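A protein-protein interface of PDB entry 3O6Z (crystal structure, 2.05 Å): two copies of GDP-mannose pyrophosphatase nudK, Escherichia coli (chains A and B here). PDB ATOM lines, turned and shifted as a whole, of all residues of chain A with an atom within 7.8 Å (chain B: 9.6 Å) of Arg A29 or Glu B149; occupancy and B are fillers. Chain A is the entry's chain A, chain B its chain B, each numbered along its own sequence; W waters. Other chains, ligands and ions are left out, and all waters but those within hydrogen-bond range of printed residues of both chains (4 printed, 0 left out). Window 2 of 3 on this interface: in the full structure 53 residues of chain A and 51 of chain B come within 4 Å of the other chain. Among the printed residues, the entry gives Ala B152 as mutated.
No position is printed for both chains. Of the 9 pairs that touch across the chains among the printed residues, none has its exchanged pair printed and touching as well.
Of the printed residues of chain B, Arg A29 touches Glu B149 (2.4 Å), Asp B150 (3.4 Å) and Glu B151 (2.8 Å). Glu B149 touches one residue of chain A. No residue of chain B comes within 4 Å of Gly A32. No residue of chain B comes within 4 Å of Glu A33. Of the printed residues of chain B, Thr A2 touches Gln B79 and Ala B152. Printed residues of chain B within 4 Å of His A37: Asp B150. Of the printed residues of chain A, Gln B79 touches Thr A2 (3.1 Å). Of the printed residues of chain B, Ile A35 touches Asp B150 (3.8 Å). Printed residues of chain A within 4 Å of Glu B151: Arg A29. Lys A30 touches none of the printed residues of chain B. Lys B99 touches none of the printed residues of chain A. The nearest residue of chain B that does not touch Arg A29 is Ala B152 (4.1 Å). The nearest residue of chain A that does not touch Glu B149 is Ile A35 (5.7 Å).
O of Ile A35 lies within hydrogen-bond range of N of Leu A27, 2.8 Å away. ND1 of His A37 lies close to NH2 of Arg A39 (3.5 Å). The guanidinium group (NH1) of Arg A29 is in salt-bridge range of the side-chain carboxylate (OE1) of Glu A33. The backbone NH (N) of Thr A2 is in hydrogen-bond range of the backbone carbonyl oxygen (O) of Thr A28, at 3.1 Å. The side-chain carboxylate (OE1) of Glu B151 sits at hydrogen-bond distance from the backbone NH (N) of Val B148, 2.9 Å away.
NE2 of His A37 sits at hydrogen-bond distance from O of Asp B150 (2.7 Å). NH2 of Arg A29 sits close to O of Glu B149 (2.4 Å). The guanidinium group (NH2) of Arg A29 is in hydrogen-bond range of the backbone carbonyl oxygen (O) of Glu B151 (2.8 Å). The side-chain carboxylate of Asp B150 lies within salt-bridge range of the guanidinium group of Arg A39, at 3.1 Å.
Water W2 lies within hydrogen-bond range of the side-chain amide oxygen of Gln B79 (2.7 Å), the side-chain carboxylate of Glu B154 (3.0 Å) and the side-chain hydroxyl of Thr A2 (3.5 Å). Water W3 bridges the guanidinium group of Arg A39 (2.7 Å) and the side-chain carboxylate of Asp B150 (3.1 Å). Water W4 lies within hydrogen-bond range of the side-chain amide nitrogen of Gln B79 (2.8 Å) and the backbone carbonyl oxygen of Gln A3 (2.9 Å). Water W1 bridges O of Glu B149 (2.8 Å) and NH1 of Arg A29 (3.1 Å).
Of the 17 printed residues of chain B, 5 touch a printed residue of chain A. Hydrophobic or aromatic side chains of chain B within 4 Å of the printed part of chain A: Ala B152. Of the 15 printed residues of chain A, 6 touch a printed residue of chain B. Printed residues of chain A that touch a printed residue of chain B: Thr A2, Leu A27, Arg A29, Ile A35, His A37 and Arg A39. Among the printed residues, 9 pairs touch across the chains.
Gln B79 touches Thr A2 (NE2 to CG2, 3.1 Å). Thr A2 touches Ala B152. CD2 of Leu A27 touches CB of Ala B152, at 3.8 Å. Arg A29 touches Asp B150 (NH2 to C, 3.4 Å). Asp B150 touches Ile A35 (CB to CG2, 3.8 Å).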
ATOM      1  N   THR A   2      -8.355 -16.411  -5.760  1.00  0.00           N
ATOM      2  CA  THR A   2      -7.684 -17.595  -5.157  1.00  0.00           C
ATOM      3  C   THR A   2      -7.019 -18.463  -6.219  1.00  0.00           C
ATOM      4  O   THR A   2      -5.862 -18.843  -6.058  1.00  0.00           O
ATOM      5  CB  THR A   2      -8.642 -18.442  -4.364  1.00  0.00           C
ATOM      6  OG1 THR A   2      -9.434 -17.599  -3.516  1.00  0.00           O
ATOM      7  CG2 THR A   2      -7.863 -19.435  -3.533  1.00  0.00           C
ATOM      8  N   GLN A   3      -7.796 -18.794  -7.260  1.00  0.00           N
ATOM      9  CA  GLN A   3      -7.346 -19.316  -8.568  1.00  0.00           C
ATOM     10  C   GLN A   3      -5.947 -19.940  -8.692  1.00  0.00           C
ATOM     11  O   GLN A   3      -5.791 -21.155  -8.593  1.00  0.00           O
ATOM     12  CB  GLN A   3      -7.501 -18.227  -9.639  1.00  0.00           C
ATOM     13  CG  GLN A   3      -8.909 -17.970 -10.105  1.00  0.00           C
ATOM     14  CD  GLN A   3      -9.202 -16.495 -10.182  1.00  0.00           C
ATOM     15  OE1 GLN A   3      -9.326 -15.827  -9.153  1.00  0.00           O
ATOM     16  NE2 GLN A   3      -9.313 -15.967 -11.408  1.00  0.00           N
ATOM     17  N   GLN A   4      -4.941 -19.100  -8.927  1.00  0.00           N
ATOM     18  CA  GLN A   4      -3.621 -19.581  -9.345  1.00  0.00           C
ATOM     19  C   GLN A   4      -2.755 -19.971  -8.168  1.00  0.00           C
ATOM     20  O   GLN A   4      -2.496 -19.143  -7.302  1.00  0.00           O
ATOM     21  CB  GLN A   4      -2.896 -18.526 -10.193  1.00  0.00           C
ATOM     22  CG  GLN A   4      -1.589 -19.025 -10.815  1.00  0.00           C
ATOM     23  CD  GLN A   4      -1.788 -20.223 -11.737  1.00  0.00           C
ATOM     24  OE1 GLN A   4      -2.729 -20.270 -12.530  1.00  0.00           O
ATOM     25  NE2 GLN A   4      -0.896 -21.195 -11.633  1.00  0.00           N
ATOM     26  N   ASP A  26       2.638 -19.650  -3.842  1.00  0.00           N
ATOM     27  CA  ASP A  26       2.088 -18.362  -4.197  1.00  0.00           C
ATOM     28  C   ASP A  26       0.639 -18.545  -4.625  1.00  0.00           C
ATOM     29  O   ASP A  26       0.299 -19.428  -5.445  1.00  0.00           O
ATOM     30  CB  ASP A  26       2.871 -17.705  -5.347  1.00  0.00           C
ATOM     31  CG  ASP A  26       4.148 -17.018  -4.887  1.00  0.00           C
ATOM     32  OD1 ASP A  26       4.313 -16.750  -3.665  1.00  0.00           O
ATOM     33  OD2 ASP A  26       4.989 -16.717  -5.773  1.00  0.00           O
ATOM     34  N   LEU A  27      -0.195 -17.659  -4.089  1.00  0.00           N
ATOM     35  CA  LEU A  27      -1.612 -17.693  -4.322  1.00  0.00           C
ATOM     36  C   LEU A  27      -2.011 -16.327  -4.851  1.00  0.00           C
ATOM     37  O   LEU A  27      -1.726 -15.290  -4.239  1.00  0.00           O
ATOM     38  CB  LEU A  27      -2.345 -18.021  -3.002  1.00  0.00           C
ATOM     39  CG  LEU A  27      -3.827 -18.411  -3.053  1.00  0.00           C
ATOM     40  CD1 LEU A  27      -4.192 -19.233  -1.837  1.00  0.00           C
ATOM     41  CD2 LEU A  27      -4.710 -17.187  -3.137  1.00  0.00           C
ATOM     42  N   THR A  28      -2.648 -16.334  -6.011  1.00  0.00           N
ATOM     43  CA  THR A  28      -3.095 -15.099  -6.637  1.00  0.00           C
ATOM     44  C   THR A  28      -4.536 -14.883  -6.200  1.00  0.00           C
ATOM     45  O   THR A  28      -5.395 -15.740  -6.416  1.00  0.00           O
ATOM     46  CB  THR A  28      -2.981 -15.169  -8.167  1.00  0.00           C
ATOM     47  OG1 THR A  28      -1.681 -15.655  -8.529  1.00  0.00           O
ATOM     48  CG2 THR A  28      -3.184 -13.793  -8.776  1.00  0.00           C
ATOM     49  N   ARG A  29      -4.793 -13.761  -5.546  1.00  0.00           N
ATOM     50  CA  ARG A  29      -6.114 -13.495  -5.001  1.00  0.00           C
ATOM     51  C   ARG A  29      -6.973 -12.972  -6.134  1.00  0.00           C
ATOM     52  O   ARG A  29      -6.462 -12.731  -7.222  1.00  0.00           O
ATOM     53  CB  ARG A  29      -6.032 -12.483  -3.867  1.00  0.00           C
ATOM     54  CG  ARG A  29      -5.470 -13.019  -2.580  1.00  0.00           C
ATOM     55  CD  ARG A  29      -5.192 -11.854  -1.659  1.00  0.00           C
ATOM     56  NE  ARG A  29      -5.348 -12.197  -0.254  1.00  0.00           N
ATOM     57  CZ  ARG A  29      -5.248 -11.319   0.740  1.00  0.00           C
ATOM     58  NH1 ARG A  29      -4.991 -10.044   0.486  1.00  0.00           N
ATOM     59  NH2 ARG A  29      -5.419 -11.718   1.991  1.00  0.00           N
ATOM     60  N   LYS A  30      -8.272 -12.800  -5.892  1.00  0.00           N
ATOM     61  CA  LYS A  30      -9.198 -12.472  -6.983  1.00  0.00           C
ATOM     62  C   LYS A  30      -8.947 -11.061  -7.518  1.00  0.00           C
ATOM     63  O   LYS A  30      -9.077 -10.812  -8.719  1.00  0.00           O
ATOM     64  CB  LYS A  30     -10.657 -12.699  -6.564  1.00  0.00           C
ATOM     65  CG  LYS A  30     -11.594 -13.007  -7.745  1.00  0.00           C
ATOM     66  CD  LYS A  30     -13.008 -13.368  -7.281  1.00  0.00           C
ATOM     67  CE  LYS A  30     -14.039 -12.557  -8.063  1.00  0.00           C
ATOM     68  NZ  LYS A  30     -15.175 -12.081  -7.204  1.00  0.00           N
ATOM     69  N   ASP A  31      -8.561 -10.157  -6.613  1.00  0.00           N
ATOM     70  CA  ASP A  31      -8.093  -8.807  -6.957  1.00  0.00           C
ATOM     71  C   ASP A  31      -6.769  -8.826  -7.728  1.00  0.00           C
ATOM     72  O   ASP A  31      -6.298  -7.782  -8.193  1.00  0.00           O
ATOM     73  CB  ASP A  31      -7.967  -7.946  -5.692  1.00  0.00           C
ATOM     74  CG  ASP A  31      -7.255  -8.665  -4.560  1.00  0.00           C
ATOM     75  OD1 ASP A  31      -7.792  -9.689  -4.048  1.00  0.00           O
ATOM     76  OD2 ASP A  31      -6.153  -8.205  -4.177  1.00  0.00           O
ATOM     77  N   GLY A  32      -6.173 -10.014  -7.852  1.00  0.00           N
ATOM     78  CA  GLY A  32      -4.989 -10.195  -8.681  1.00  0.00           C
ATOM     79  C   GLY A  32      -3.711 -10.067  -7.884  1.00  0.00           C
ATOM     80  O   GLY A  32      -2.617 -10.208  -8.429  1.00  0.00           O
ATOM     81  N   GLU A  33      -3.858  -9.793  -6.589  1.00  0.00           N
ATOM     82  CA  GLU A  33      -2.722  -9.667  -5.690  1.00  0.00           C
ATOM     83  C   GLU A  33      -2.103 -11.042  -5.446  1.00  0.00           C
ATOM     84  O   GLU A  33      -2.825 -12.042  -5.329  1.00  0.00           O
ATOM     85  CB  GLU A  33      -3.186  -9.010  -4.389  1.00  0.00           C
ATOM     86  CG  GLU A  33      -2.289  -9.159  -3.173  1.00  0.00           C
ATOM     87  CD  GLU A  33      -2.900  -8.504  -1.949  1.00  0.00           C
ATOM     88  OE1 GLU A  33      -3.881  -9.053  -1.421  1.00  0.00           O
ATOM     89  OE2 GLU A  33      -2.418  -7.439  -1.512  1.00  0.00           O
ATOM     90  N   VAL A  34      -0.769 -11.091  -5.391  1.00  0.00           N
ATOM     91  CA  VAL A  34      -0.057 -12.337  -5.133  1.00  0.00           C
ATOM     92  C   VAL A  34       0.454 -12.404  -3.687  1.00  0.00           C
ATOM     93  O   VAL A  34       1.229 -11.532  -3.236  1.00  0.00           O
ATOM     94  CB  VAL A  34       1.093 -12.610  -6.152  1.00  0.00           C
ATOM     95  CG1 VAL A  34       1.804 -13.947  -5.811  1.00  0.00           C
ATOM     96  CG2 VAL A  34       0.552 -12.617  -7.592  1.00  0.00           C
ATOM     97  N   ILE A  35      -0.026 -13.434  -2.976  1.00  0.00           N
ATOM     98  CA  ILE A  35       0.330 -13.677  -1.578  1.00  0.00           C
ATOM     99  C   ILE A  35       1.119 -14.958  -1.488  1.00  0.00           C
ATOM    100  O   ILE A  35       0.710 -15.993  -2.017  1.00  0.00           O
ATOM    101  CB  ILE A  35      -0.933 -13.717  -0.620  1.00  0.00           C
ATOM    102  CG1 ILE A  35      -1.655 -12.363  -0.626  1.00  0.00           C
ATOM    103  CG2 ILE A  35      -0.549 -14.084   0.818  1.00  0.00           C
ATOM    104  CD1 ILE A  35      -0.845 -11.213  -0.119  1.00  0.00           C
ATOM    105  N   HIS A  37       1.944 -17.840   0.846  1.00  0.00           N
ATOM    106  CA  HIS A  37       1.601 -18.567   2.070  1.00  0.00           C
ATOM    107  C   HIS A  37       2.724 -19.510   2.428  1.00  0.00           C
ATOM    108  O   HIS A  37       3.312 -20.129   1.545  1.00  0.00           O
ATOM    109  CB  HIS A  37       0.375 -19.432   1.833  1.00  0.00           C
ATOM    110  CG  HIS A  37      -0.933 -18.696   1.854  1.00  0.00           C
ATOM    111  ND1 HIS A  37      -2.142 -19.356   1.769  1.00  0.00           N
ATOM    112  CD2 HIS A  37      -1.230 -17.382   1.970  1.00  0.00           C
ATOM    113  CE1 HIS A  37      -3.128 -18.478   1.817  1.00  0.00           C
ATOM    114  NE2 HIS A  37      -2.603 -17.272   1.940  1.00  0.00           N
ATOM    115  N   ARG A  39       2.770 -22.784   5.033  1.00  0.00           N
ATOM    116  CA  ARG A  39       1.784 -23.566   5.771  1.00  0.00           C
ATOM    117  C   ARG A  39       2.383 -24.892   6.182  1.00  0.00           C
ATOM    118  O   ARG A  39       2.971 -25.595   5.344  1.00  0.00           O
ATOM    119  CB  ARG A  39       0.557 -23.829   4.879  1.00  0.00           C
ATOM    120  CG  ARG A  39      -0.361 -22.642   4.596  1.00  0.00           C
ATOM    121  CD  ARG A  39      -1.148 -22.169   5.842  1.00  0.00           C
ATOM    122  NE  ARG A  39      -2.071 -21.072   5.518  1.00  0.00           N
ATOM    123  CZ  ARG A  39      -1.724 -19.788   5.469  1.00  0.00           C
ATOM    124  NH1 ARG A  39      -0.473 -19.432   5.731  1.00  0.00           N
ATOM    125  NH2 ARG A  39      -2.628 -18.855   5.172  1.00  0.00           N
ATOM    126  N   TYR B  17       4.881 -22.308  15.187  1.00  0.00           N
ATOM    127  CA  TYR B  17       3.704 -21.648  15.735  1.00  0.00           C
ATOM    128  C   TYR B  17       2.966 -22.757  16.436  1.00  0.00           C
ATOM    129  O   TYR B  17       2.630 -22.651  17.622  1.00  0.00           O
ATOM    130  CB  TYR B  17       2.828 -21.022  14.631  1.00  0.00           C
ATOM    131  CG  TYR B  17       1.729 -20.130  15.175  1.00  0.00           C
ATOM    132  CD1 TYR B  17       1.990 -18.804  15.538  1.00  0.00           C
ATOM    133  CD2 TYR B  17       0.437 -20.621  15.367  1.00  0.00           C
ATOM    134  CE1 TYR B  17       0.982 -17.982  16.063  1.00  0.00           C
ATOM    135  CE2 TYR B  17      -0.569 -19.819  15.896  1.00  0.00           C
ATOM    136  CZ  TYR B  17      -0.295 -18.503  16.239  1.00  0.00           C
ATOM    137  OH  TYR B  17      -1.292 -17.707  16.758  1.00  0.00           O
ATOM    138  N   GLN B  79      -9.113 -26.537  -3.549  1.00  0.00           N
ATOM    139  CA  GLN B  79     -10.256 -25.774  -3.069  1.00  0.00           C
ATOM    140  C   GLN B  79     -11.207 -26.651  -2.291  1.00  0.00           C
ATOM    141  O   GLN B  79     -11.494 -27.781  -2.686  1.00  0.00           O
ATOM    142  CB  GLN B  79     -10.986 -25.072  -4.201  1.00  0.00           C
ATOM    143  CG  GLN B  79     -10.113 -24.119  -5.005  1.00  0.00           C
ATOM    144  CD  GLN B  79      -9.796 -22.834  -4.245  1.00  0.00           C
ATOM    145  OE1 GLN B  79     -10.594 -22.371  -3.421  1.00  0.00           O
ATOM    146  NE2 GLN B  79      -8.644 -22.218  -4.566  1.00  0.00           N
ATOM    147  N   ASP B  89      -7.264 -19.084  19.253  1.00  0.00           N
ATOM    148  CA  ASP B  89      -6.243 -18.029  19.440  1.00  0.00           C
ATOM    149  C   ASP B  89      -6.546 -17.237  20.727  1.00  0.00           C
ATOM    150  O   ASP B  89      -6.611 -15.995  20.716  1.00  0.00           O
ATOM    151  CB  ASP B  89      -6.209 -17.107  18.197  1.00  0.00           C
ATOM    152  CG  ASP B  89      -5.019 -16.129  18.192  1.00  0.00           C
ATOM    153  OD1 ASP B  89      -3.931 -16.482  18.696  1.00  0.00           O
ATOM    154  OD2 ASP B  89      -5.176 -15.006  17.658  1.00  0.00           O
ATOM    155  N   LYS B  99     -16.497 -13.168  15.462  1.00  0.00           N
ATOM    156  CA  LYS B  99     -15.325 -12.581  14.789  1.00  0.00           C
ATOM    157  C   LYS B  99     -15.000 -13.276  13.468  1.00  0.00           C
ATOM    158  O   LYS B  99     -14.964 -12.631  12.436  1.00  0.00           O
ATOM    159  CB  LYS B  99     -14.125 -12.655  15.734  1.00  0.00           C
ATOM    160  CG  LYS B  99     -12.888 -11.914  15.312  1.00  0.00           C
ATOM    161  CD  LYS B  99     -11.941 -11.857  16.510  1.00  0.00           C
ATOM    162  CE  LYS B  99     -10.513 -11.543  16.107  1.00  0.00           C
ATOM    163  NZ  LYS B  99      -9.631 -11.406  17.314  1.00  0.00           N
ATOM    164  N   GLU B 100     -14.737 -14.586  13.499  1.00  0.00           N
ATOM    165  CA  GLU B 100     -14.546 -15.355  12.248  1.00  0.00           C
ATOM    166  C   GLU B 100     -15.708 -15.224  11.258  1.00  0.00           C
ATOM    167  O   GLU B 100     -15.487 -15.110  10.033  1.00  0.00           O
ATOM    168  CB  GLU B 100     -14.271 -16.855  12.508  1.00  0.00           C
ATOM    169  CG  GLU B 100     -12.966 -17.202  13.229  1.00  0.00           C
ATOM    170  CD  GLU B 100     -11.697 -16.903  12.427  1.00  0.00           C
ATOM    171  OE1 GLU B 100     -11.737 -16.879  11.200  1.00  0.00           O
ATOM    172  OE2 GLU B 100     -10.629 -16.688  13.027  1.00  0.00           O
ATOM    173  N   GLU B 103     -15.595 -11.734   9.492  1.00  0.00           N
ATOM    174  CA  GLU B 103     -14.379 -11.636   8.666  1.00  0.00           C
ATOM    175  C   GLU B 103     -14.511 -12.458   7.402  1.00  0.00           C
ATOM    176  O   GLU B 103     -14.283 -11.954   6.305  1.00  0.00           O
ATOM    177  CB  GLU B 103     -13.160 -12.097   9.437  1.00  0.00           C
ATOM    178  CG  GLU B 103     -12.798 -11.168  10.607  1.00  0.00           C
ATOM    179  CD  GLU B 103     -11.557 -11.656  11.349  1.00  0.00           C
ATOM    180  OE1 GLU B 103     -11.155 -12.832  11.201  1.00  0.00           O
ATOM    181  OE2 GLU B 103     -10.995 -10.848  12.095  1.00  0.00           O
ATOM    182  N   GLU B 104     -14.901 -13.718   7.574  1.00  0.00           N
ATOM    183  CA  GLU B 104     -14.988 -14.668   6.476  1.00  0.00           C
ATOM    184  C   GLU B 104     -16.256 -14.566   5.641  1.00  0.00           C
ATOM    185  O   GLU B 104     -16.188 -14.685   4.404  1.00  0.00           O
ATOM    186  CB  GLU B 104     -14.750 -16.090   6.987  1.00  0.00           C
ATOM    187  CG  GLU B 104     -13.464 -16.198   7.840  1.00  0.00           C
ATOM    188  CD  GLU B 104     -12.989 -17.626   8.036  1.00  0.00           C
ATOM    189  OE1 GLU B 104     -13.742 -18.567   7.749  1.00  0.00           O
ATOM    190  OE2 GLU B 104     -11.843 -17.820   8.509  1.00  0.00           O
ATOM    191  N   GLY B 145     -17.282 -10.177   3.303  1.00  0.00           N
ATOM    192  CA  GLY B 145     -16.485 -11.293   3.864  1.00  0.00           C
ATOM    193  C   GLY B 145     -15.146 -11.450   3.149  1.00  0.00           C
ATOM    194  O   GLY B 145     -14.537 -10.451   2.770  1.00  0.00           O
ATOM    195  N   GLY B 146     -14.705 -12.702   2.929  1.00  0.00           N
ATOM    196  CA  GLY B 146     -13.456 -12.984   2.175  1.00  0.00           C
ATOM    197  C   GLY B 146     -12.180 -13.166   2.994  1.00  0.00           C
ATOM    198  O   GLY B 146     -11.088 -13.439   2.443  1.00  0.00           O
ATOM    199  N   GLY B 147     -12.312 -13.051   4.317  1.00  0.00           N
ATOM    200  CA  GLY B 147     -11.175 -13.135   5.229  1.00  0.00           C
ATOM    201  C   GLY B 147     -10.357 -11.848   5.334  1.00  0.00           C
ATOM    202  O   GLY B 147     -10.666 -10.843   4.690  1.00  0.00           O
ATOM    203  N   VAL B 148      -9.318 -11.906   6.165  1.00  0.00           N
ATOM    204  CA  VAL B 148      -8.419 -10.807   6.450  1.00  0.00           C
ATOM    205  C   VAL B 148      -6.994 -11.339   6.399  1.00  0.00           C
ATOM    206  O   VAL B 148      -6.787 -12.546   6.255  1.00  0.00           O
ATOM    207  CB  VAL B 148      -8.659 -10.236   7.865  1.00  0.00           C
ATOM    208  CG1 VAL B 148     -10.009  -9.561   7.943  1.00  0.00           C
ATOM    209  CG2 VAL B 148      -8.527 -11.323   8.904  1.00  0.00           C
ATOM    210  N   GLU B 149      -6.030 -10.441   6.546  1.00  0.00           N
ATOM    211  CA  GLU B 149      -4.595 -10.782   6.535  1.00  0.00           C
ATOM    212  C   GLU B 149      -4.293 -11.561   5.222  1.00  0.00           C
ATOM    213  O   GLU B 149      -4.627 -11.069   4.139  1.00  0.00           O
ATOM    214  CB  GLU B 149      -4.203 -11.521   7.834  1.00  0.00           C
ATOM    215  CG  GLU B 149      -4.451 -10.685   9.089  1.00  0.00           C
ATOM    216  CD  GLU B 149      -4.144 -11.406  10.397  1.00  0.00           C
ATOM    217  OE1 GLU B 149      -3.850 -12.620  10.416  1.00  0.00           O
ATOM    218  OE2 GLU B 149      -4.186 -10.730  11.432  1.00  0.00           O
ATOM    219  N   ASP B 150      -3.706 -12.754   5.314  1.00  0.00           N
ATOM    220  CA  ASP B 150      -3.400 -13.554   4.111  1.00  0.00           C
ATOM    221  C   ASP B 150      -4.535 -14.525   3.649  1.00  0.00           C
ATOM    222  O   ASP B 150      -4.326 -15.391   2.789  1.00  0.00           O
ATOM    223  CB  ASP B 150      -2.055 -14.295   4.312  1.00  0.00           C
ATOM    224  CG  ASP B 150      -2.121 -15.390   5.337  1.00  0.00           C
ATOM    225  OD1 ASP B 150      -3.125 -15.552   6.032  1.00  0.00           O
ATOM    226  OD2 ASP B 150      -1.136 -16.136   5.465  1.00  0.00           O
ATOM    227  N   GLU B 151      -5.726 -14.408   4.244  1.00  0.00           N
ATOM    228  CA  GLU B 151      -6.817 -15.308   3.873  1.00  0.00           C
ATOM    229  C   GLU B 151      -7.338 -14.955   2.481  1.00  0.00           C
ATOM    230  O   GLU B 151      -7.329 -13.794   2.081  1.00  0.00           O
ATOM    231  CB  GLU B 151      -7.960 -15.238   4.880  1.00  0.00           C
ATOM    232  CG  GLU B 151      -7.707 -15.991   6.172  1.00  0.00           C
ATOM    233  CD  GLU B 151      -8.791 -15.773   7.168  1.00  0.00           C
ATOM    234  OE1 GLU B 151      -9.270 -14.608   7.331  1.00  0.00           O
ATOM    235  OE2 GLU B 151      -9.160 -16.762   7.813  1.00  0.00           O
ATOM    236  N   ALA B 152      -7.787 -15.981   1.750  1.00  0.00           N
ATOM    237  CA  ALA B 152      -8.374 -15.788   0.430  1.00  0.00           C
ATOM    238  C   ALA B 152      -9.604 -16.681   0.349  1.00  0.00           C
ATOM    239  O   ALA B 152      -9.526 -17.868   0.009  1.00  0.00           O
ATOM    240  CB  ALA B 152      -7.373 -16.105  -0.666  1.00  0.00           C
ATOM    241  N   ILE B 153     -10.743 -16.090   0.691  1.00  0.00           N
ATOM    242  CA  ILE B 153     -11.955 -16.853   0.928  1.00  0.00           C
ATOM    243  C   ILE B 153     -13.088 -16.434  -0.008  1.00  0.00           C
ATOM    244  O   ILE B 153     -13.386 -15.242  -0.166  1.00  0.00           O
ATOM    245  CB  ILE B 153     -12.392 -16.719   2.407  1.00  0.00           C
ATOM    246  CG1 ILE B 153     -11.427 -17.492   3.323  1.00  0.00           C
ATOM    247  CG2 ILE B 153     -13.842 -17.181   2.599  1.00  0.00           C
ATOM    248  CD1 ILE B 153     -11.627 -17.264   4.803  1.00  0.00           C
ATOM    249  N   GLU B 154     -13.714 -17.437  -0.610  1.00  0.00           N
ATOM    250  CA  GLU B 154     -14.896 -17.275  -1.437  1.00  0.00           C
ATOM    251  C   GLU B 154     -16.140 -17.560  -0.567  1.00  0.00           C
ATOM    252  O   GLU B 154     -16.198 -18.578   0.130  1.00  0.00           O
ATOM    253  CB  GLU B 154     -14.809 -18.304  -2.561  1.00  0.00           C
ATOM    254  CG  GLU B 154     -15.754 -18.077  -3.719  1.00  0.00           C
ATOM    255  CD  GLU B 154     -15.694 -19.189  -4.718  1.00  0.00           C
ATOM    256  OE1 GLU B 154     -14.820 -20.074  -4.594  1.00  0.00           O
ATOM    257  OE2 GLU B 154     -16.523 -19.179  -5.641  1.00  0.00           O
HETATM  258  O   HOH W   1      -5.203  -8.478   3.157  1.00  0.00           O
HETATM  259  O   HOH W   2     -11.885 -20.051  -3.782  1.00  0.00           O
HETATM  260  O   HOH W   3       1.569 -17.645   5.473  1.00  0.00           O
HETATM  261  O   HOH W   4      -7.050 -22.932  -6.704  1.00  0.00           O
